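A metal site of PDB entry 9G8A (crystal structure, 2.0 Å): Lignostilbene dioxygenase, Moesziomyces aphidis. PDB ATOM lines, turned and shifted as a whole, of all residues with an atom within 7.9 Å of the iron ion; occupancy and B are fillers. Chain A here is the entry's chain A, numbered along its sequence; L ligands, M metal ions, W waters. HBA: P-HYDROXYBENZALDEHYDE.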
ATOM      1  N   LEU A  49       2.787 -33.461  23.095  1.00  0.00           N
ATOM      2  CA  LEU A  49       1.981 -32.781  22.086  1.00  0.00           C
ATOM      3  C   LEU A  49       0.654 -33.484  21.761  1.00  0.00           C
ATOM      4  O   LEU A  49      -0.325 -32.789  21.453  1.00  0.00           O
ATOM      5  CB  LEU A  49       2.755 -32.326  20.837  1.00  0.00           C
ATOM      6  CG  LEU A  49       3.590 -31.036  20.932  1.00  0.00           C
ATOM      7  CD1 LEU A  49       4.354 -30.926  19.629  1.00  0.00           C
ATOM      8  CD2 LEU A  49       2.789 -29.748  21.133  1.00  0.00           C
ATOM      9  N   THR A 164      13.431 -31.474  20.200  1.00  0.00           N
ATOM     10  CA  THR A 164      12.572 -31.041  19.113  1.00  0.00           C
ATOM     11  C   THR A 164      12.811 -31.846  17.824  1.00  0.00           C
ATOM     12  O   THR A 164      11.829 -32.330  17.237  1.00  0.00           O
ATOM     13  CB  THR A 164      12.633 -29.531  18.892  1.00  0.00           C
ATOM     14  OG1 THR A 164      12.362 -28.895  20.141  1.00  0.00           O
ATOM     15  CG2 THR A 164      11.632 -29.023  17.863  1.00  0.00           C
ATOM     16  N   ASN A 165      14.072 -31.922  17.371  1.00  0.00           N
ATOM     17  CA  ASN A 165      14.449 -32.483  16.079  1.00  0.00           C
ATOM     18  C   ASN A 165      15.894 -32.995  16.125  1.00  0.00           C
ATOM     19  O   ASN A 165      16.645 -32.647  17.029  1.00  0.00           O
ATOM     20  CB  ASN A 165      14.107 -31.531  14.916  1.00  0.00           C
ATOM     21  CG  ASN A 165      14.114 -32.169  13.534  1.00  0.00           C
ATOM     22  OD1 ASN A 165      14.069 -33.402  13.365  1.00  0.00           O
ATOM     23  ND2 ASN A 165      14.144 -31.327  12.520  1.00  0.00           N
ATOM     24  N   GLU A 178      15.366 -24.909  19.871  1.00  0.00           N
ATOM     25  CA  GLU A 178      15.569 -23.543  19.373  1.00  0.00           C
ATOM     26  C   GLU A 178      16.146 -22.557  20.398  1.00  0.00           C
ATOM     27  O   GLU A 178      16.626 -21.499  19.959  1.00  0.00           O
ATOM     28  CB  GLU A 178      14.358 -22.953  18.624  1.00  0.00           C
ATOM     29  CG  GLU A 178      13.125 -22.688  19.488  1.00  0.00           C
ATOM     30  CD  GLU A 178      11.934 -22.822  18.575  1.00  0.00           C
ATOM     31  OE1 GLU A 178      11.545 -23.972  18.203  1.00  0.00           O
ATOM     32  OE2 GLU A 178      11.416 -21.768  18.200  1.00  0.00           O
ATOM     33  N   ALA A 207      15.805 -25.703  15.483  1.00  0.00           N
ATOM     34  CA  ALA A 207      15.612 -27.138  15.345  1.00  0.00           C
ATOM     35  C   ALA A 207      15.126 -27.514  13.942  1.00  0.00           C
ATOM     36  O   ALA A 207      14.980 -28.700  13.616  1.00  0.00           O
ATOM     37  CB  ALA A 207      14.743 -27.658  16.448  1.00  0.00           C
ATOM     38  N   HIS A 208      14.970 -26.511  13.076  1.00  0.00           N
ATOM     39  CA  HIS A 208      14.583 -26.696  11.695  1.00  0.00           C
ATOM     40  C   HIS A 208      15.643 -26.216  10.704  1.00  0.00           C
ATOM     41  O   HIS A 208      15.283 -25.433   9.822  1.00  0.00           O
ATOM     42  CB  HIS A 208      13.185 -26.110  11.492  1.00  0.00           C
ATOM     43  CG  HIS A 208      12.137 -26.993  12.055  1.00  0.00           C
ATOM     44  ND1 HIS A 208      11.876 -28.237  11.554  1.00  0.00           N
ATOM     45  CD2 HIS A 208      11.319 -26.806  13.097  1.00  0.00           C
ATOM     46  CE1 HIS A 208      10.920 -28.782  12.269  1.00  0.00           C
ATOM     47  NE2 HIS A 208      10.576 -27.936  13.216  1.00  0.00           N
ATOM     48  N   LYS A 210      17.829 -26.920   7.208  1.00  0.00           N
ATOM     49  CA  LYS A 210      17.498 -27.621   5.974  1.00  0.00           C
ATOM     50  C   LYS A 210      18.788 -28.016   5.282  1.00  0.00           C
ATOM     51  O   LYS A 210      19.670 -27.160   5.105  1.00  0.00           O
ATOM     52  CB  LYS A 210      16.537 -26.816   5.085  1.00  0.00           C
ATOM     53  CG  LYS A 210      15.285 -26.232   5.738  1.00  0.00           C
ATOM     54  CD  LYS A 210      14.251 -27.178   6.362  1.00  0.00           C
ATOM     55  CE  LYS A 210      13.192 -26.375   7.083  1.00  0.00           C
ATOM     56  NZ  LYS A 210      12.185 -27.258   7.675  1.00  0.00           N
ATOM     57  N   HIS A 259       9.986 -20.587  14.606  1.00  0.00           N
ATOM     58  CA  HIS A 259      10.144 -22.021  14.799  1.00  0.00           C
ATOM     59  C   HIS A 259      10.747 -22.716  13.570  1.00  0.00           C
ATOM     60  O   HIS A 259      11.677 -23.537  13.716  1.00  0.00           O
ATOM     61  CB  HIS A 259       8.824 -22.613  15.295  1.00  0.00           C
ATOM     62  CG  HIS A 259       8.910 -24.086  15.456  1.00  0.00           C
ATOM     63  ND1 HIS A 259       9.720 -24.649  16.423  1.00  0.00           N
ATOM     64  CD2 HIS A 259       8.397 -25.115  14.753  1.00  0.00           C
ATOM     65  CE1 HIS A 259       9.672 -25.964  16.321  1.00  0.00           C
ATOM     66  NE2 HIS A 259       8.848 -26.255  15.336  1.00  0.00           N
ATOM     67  N   ASP A 260      10.189 -22.416  12.392  1.00  0.00           N
ATOM     68  CA  ASP A 260      10.446 -23.085  11.131  1.00  0.00           C
ATOM     69  C   ASP A 260      10.753 -22.057  10.040  1.00  0.00           C
ATOM     70  O   ASP A 260      10.677 -20.838  10.254  1.00  0.00           O
ATOM     71  CB  ASP A 260       9.365 -24.140  10.873  1.00  0.00           C
ATOM     72  CG  ASP A 260       9.694 -25.271   9.916  1.00  0.00           C
ATOM     73  OD1 ASP A 260      10.839 -25.370   9.387  1.00  0.00           O
ATOM     74  OD2 ASP A 260       8.775 -26.057   9.661  1.00  0.00           O
ATOM     75  N   TRP A 273       5.784 -16.750  13.703  1.00  0.00           N
ATOM     76  CA  TRP A 273       4.528 -16.940  14.420  1.00  0.00           C
ATOM     77  C   TRP A 273       4.126 -15.654  15.161  1.00  0.00           C
ATOM     78  O   TRP A 273       5.023 -14.975  15.677  1.00  0.00           O
ATOM     79  CB  TRP A 273       4.580 -18.128  15.385  1.00  0.00           C
ATOM     80  CG  TRP A 273       4.802 -19.495  14.796  1.00  0.00           C
ATOM     81  CD1 TRP A 273       4.781 -19.892  13.484  1.00  0.00           C
ATOM     82  CD2 TRP A 273       5.018 -20.702  15.572  1.00  0.00           C
ATOM     83  NE1 TRP A 273       5.028 -21.235  13.384  1.00  0.00           N
ATOM     84  CE2 TRP A 273       5.166 -21.767  14.641  1.00  0.00           C
ATOM     85  CE3 TRP A 273       5.108 -20.997  16.954  1.00  0.00           C
ATOM     86  CZ2 TRP A 273       5.378 -23.100  15.061  1.00  0.00           C
ATOM     87  CZ3 TRP A 273       5.314 -22.308  17.370  1.00  0.00           C
ATOM     88  CH2 TRP A 273       5.454 -23.336  16.422  1.00  0.00           C
ATOM     89  N   ILE A 323       2.383 -23.639  11.313  1.00  0.00           N
ATOM     90  CA  ILE A 323       3.217 -24.308  12.313  1.00  0.00           C
ATOM     91  C   ILE A 323       4.497 -24.795  11.652  1.00  0.00           C
ATOM     92  O   ILE A 323       5.584 -24.433  12.112  1.00  0.00           O
ATOM     93  CB  ILE A 323       2.483 -25.374  13.150  1.00  0.00           C
ATOM     94  CG1 ILE A 323       1.204 -24.806  13.799  1.00  0.00           C
ATOM     95  CG2 ILE A 323       3.414 -26.022  14.184  1.00  0.00           C
ATOM     96  CD1 ILE A 323       0.171 -25.864  14.145  1.00  0.00           C
ATOM     97  N   HIS A 324       4.352 -25.602  10.580  1.00  0.00           N
ATOM     98  CA  HIS A 324       5.449 -26.224   9.870  1.00  0.00           C
ATOM     99  C   HIS A 324       5.283 -26.072   8.355  1.00  0.00           C
ATOM    100  O   HIS A 324       4.174 -26.245   7.850  1.00  0.00           O
ATOM    101  CB  HIS A 324       5.563 -27.705  10.240  1.00  0.00           C
ATOM    102  CG  HIS A 324       6.061 -27.942  11.616  1.00  0.00           C
ATOM    103  ND1 HIS A 324       5.289 -28.551  12.584  1.00  0.00           N
ATOM    104  CD2 HIS A 324       7.258 -27.711  12.170  1.00  0.00           C
ATOM    105  CE1 HIS A 324       5.987 -28.656  13.686  1.00  0.00           C
ATOM    106  NE2 HIS A 324       7.184 -28.129  13.451  1.00  0.00           N
ATOM    107  N   THR A 325       6.418 -25.809   7.684  1.00  0.00           N
ATOM    108  CA  THR A 325       6.568 -25.870   6.240  1.00  0.00           C
ATOM    109  C   THR A 325       6.716 -27.332   5.791  1.00  0.00           C
ATOM    110  O   THR A 325       7.361 -28.129   6.489  1.00  0.00           O
ATOM    111  CB  THR A 325       7.733 -25.011   5.725  1.00  0.00           C
ATOM    112  OG1 THR A 325       8.942 -25.488   6.323  1.00  0.00           O
ATOM    113  CG2 THR A 325       7.603 -23.527   6.041  1.00  0.00           C
ATOM    114  N   PHE A 348      -1.027 -23.273  20.227  1.00  0.00           N
ATOM    115  CA  PHE A 348      -0.423 -23.389  21.555  1.00  0.00           C
ATOM    116  C   PHE A 348      -1.233 -22.579  22.584  1.00  0.00           C
ATOM    117  O   PHE A 348      -0.673 -21.603  23.115  1.00  0.00           O
ATOM    118  CB  PHE A 348       1.046 -22.938  21.403  1.00  0.00           C
ATOM    119  CG  PHE A 348       2.137 -23.851  20.841  1.00  0.00           C
ATOM    120  CD1 PHE A 348       1.859 -25.103  20.264  1.00  0.00           C
ATOM    121  CD2 PHE A 348       3.468 -23.398  20.881  1.00  0.00           C
ATOM    122  CE1 PHE A 348       2.904 -25.920  19.795  1.00  0.00           C
ATOM    123  CE2 PHE A 348       4.508 -24.188  20.368  1.00  0.00           C
ATOM    124  CZ  PHE A 348       4.223 -25.457  19.828  1.00  0.00           C
ATOM    125  N   GLU A 399      -0.602 -31.425   9.908  1.00  0.00           N
ATOM    126  CA  GLU A 399       0.591 -31.112  10.674  1.00  0.00           C
ATOM    127  C   GLU A 399       1.758 -32.014  10.272  1.00  0.00           C
ATOM    128  O   GLU A 399       1.612 -32.882   9.412  1.00  0.00           O
ATOM    129  CB  GLU A 399       0.368 -30.963  12.187  1.00  0.00           C
ATOM    130  CG  GLU A 399       0.574 -29.530  12.677  1.00  0.00           C
ATOM    131  CD  GLU A 399       1.971 -29.015  12.371  1.00  0.00           C
ATOM    132  OE1 GLU A 399       2.901 -29.536  12.993  1.00  0.00           O
ATOM    133  OE2 GLU A 399       2.170 -28.202  11.453  1.00  0.00           O
ATOM    134  N   PHE A 400       2.947 -31.706  10.822  1.00  0.00           N
ATOM    135  CA  PHE A 400       4.196 -32.456  10.675  1.00  0.00           C
ATOM    136  C   PHE A 400       4.426 -32.901   9.221  1.00  0.00           C
ATOM    137  O   PHE A 400       4.573 -34.115   8.983  1.00  0.00           O
ATOM    138  CB  PHE A 400       4.169 -33.537  11.770  1.00  0.00           C
ATOM    139  CG  PHE A 400       4.308 -33.089  13.222  1.00  0.00           C
ATOM    140  CD1 PHE A 400       5.527 -32.596  13.711  1.00  0.00           C
ATOM    141  CD2 PHE A 400       3.242 -33.274  14.132  1.00  0.00           C
ATOM    142  CE1 PHE A 400       5.684 -32.211  15.053  1.00  0.00           C
ATOM    143  CE2 PHE A 400       3.406 -32.919  15.472  1.00  0.00           C
ATOM    144  CZ  PHE A 400       4.613 -32.373  15.929  1.00  0.00           C
ATOM    145  N   PHE A 432      -2.649 -30.902  17.294  1.00  0.00           N
ATOM    146  CA  PHE A 432      -1.618 -31.868  17.679  1.00  0.00           C
ATOM    147  C   PHE A 432      -2.188 -33.168  18.258  1.00  0.00           C
ATOM    148  O   PHE A 432      -1.433 -34.126  18.450  1.00  0.00           O
ATOM    149  CB  PHE A 432      -0.587 -31.230  18.609  1.00  0.00           C
ATOM    150  CG  PHE A 432       0.244 -30.117  17.997  1.00  0.00           C
ATOM    151  CD1 PHE A 432       1.316 -30.401  17.136  1.00  0.00           C
ATOM    152  CD2 PHE A 432      -0.039 -28.770  18.315  1.00  0.00           C
ATOM    153  CE1 PHE A 432       2.084 -29.375  16.592  1.00  0.00           C
ATOM    154  CE2 PHE A 432       0.727 -27.740  17.761  1.00  0.00           C
ATOM    155  CZ  PHE A 432       1.793 -28.039  16.907  1.00  0.00           C
ATOM    156  N   GLU A 461       4.568 -38.051  12.958  1.00  0.00           N
ATOM    157  CA  GLU A 461       5.192 -37.490  11.768  1.00  0.00           C
ATOM    158  C   GLU A 461       5.756 -38.574  10.835  1.00  0.00           C
ATOM    159  O   GLU A 461       6.576 -39.394  11.278  1.00  0.00           O
ATOM    160  CB  GLU A 461       6.273 -36.487  12.158  1.00  0.00           C
ATOM    161  CG  GLU A 461       7.013 -35.892  10.952  1.00  0.00           C
ATOM    162  CD  GLU A 461       8.271 -35.166  11.375  1.00  0.00           C
ATOM    163  OE1 GLU A 461       9.090 -35.788  12.074  1.00  0.00           O
ATOM    164  OE2 GLU A 461       8.451 -34.018  10.969  1.00  0.00           O
ATOM    165  N   ILE A 517       7.930 -35.298  18.770  1.00  0.00           N
ATOM    166  CA  ILE A 517       7.862 -34.060  18.006  1.00  0.00           C
ATOM    167  C   ILE A 517       8.297 -34.423  16.581  1.00  0.00           C
ATOM    168  O   ILE A 517       7.451 -34.900  15.806  1.00  0.00           O
ATOM    169  CB  ILE A 517       8.563 -32.874  18.734  1.00  0.00           C
ATOM    170  CG1 ILE A 517       8.095 -32.733  20.229  1.00  0.00           C
ATOM    171  CG2 ILE A 517       8.337 -31.578  17.949  1.00  0.00           C
ATOM    172  CD1 ILE A 517       8.743 -31.639  21.076  1.00  0.00           C
ATOM    173  N   HIS A 518       9.600 -34.294  16.276  1.00  0.00           N
ATOM    174  CA  HIS A 518      10.138 -34.667  14.968  1.00  0.00           C
ATOM    175  C   HIS A 518      10.906 -35.971  15.041  1.00  0.00           C
ATOM    176  O   HIS A 518      11.387 -36.369  16.112  1.00  0.00           O
ATOM    177  CB  HIS A 518      10.957 -33.543  14.318  1.00  0.00           C
ATOM    178  CG  HIS A 518      10.111 -32.368  14.021  1.00  0.00           C
ATOM    179  ND1 HIS A 518       9.249 -32.271  12.948  1.00  0.00           N
ATOM    180  CD2 HIS A 518       9.958 -31.262  14.732  1.00  0.00           C
ATOM    181  CE1 HIS A 518       8.607 -31.118  13.003  1.00  0.00           C
ATOM    182  NE2 HIS A 518       9.002 -30.500  14.095  1.00  0.00           N
HETATM  183  C1' HBA L   1       6.632 -27.077  17.869  1.00  0.00           C
HETATM  184  O1' HBA L   1       6.427 -28.168  17.347  1.00  0.00           O
HETATM  185  C1  HBA L   1       7.648 -26.778  18.897  1.00  0.00           C
HETATM  186  C2  HBA L   1       8.436 -27.780  19.477  1.00  0.00           C
HETATM  187  C3  HBA L   1       9.404 -27.486  20.433  1.00  0.00           C
HETATM  188  C4  HBA L   1       9.615 -26.149  20.779  1.00  0.00           C
HETATM  189  C5  HBA L   1       8.884 -25.123  20.172  1.00  0.00           C
HETATM  190  C6  HBA L   1       7.899 -25.432  19.244  1.00  0.00           C
HETATM  191  O4  HBA L   1      10.595 -25.811  21.685  1.00  0.00           O
HETATM  192 FE    FE M   1       8.915 -28.397  14.661  1.00  0.00          FE
HETATM  193  O   HOH W   1       8.726 -28.934  16.376  1.00  0.00           O
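The backbone NH (N) of His 518 sits at hydrogen-bond distance from the backbone carbonyl oxygen (O) of Thr 164.
A ring nitrogen (ND1) of His 518 sits at hydrogen-bond distance from the side-chain carboxylate (OE2) of Glu 461, at 2.8 Å.
OE1 of Glu 399 lies within hydrogen-bond range of ND1 of His 324 (2.6 Å).
A ring nitrogen (ND1) of His 259 lies within hydrogen-bond range of the side-chain carboxylate (OE1) of Glu 178.
The iron ion is bound by water W1 (1.8 Å), NE2 of His 324 (2.1 Å), NE2 of His 518 (2.2 Å), NE2 of His 259 (2.2 Å) and NE2 of His 208 (2.2 Å).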
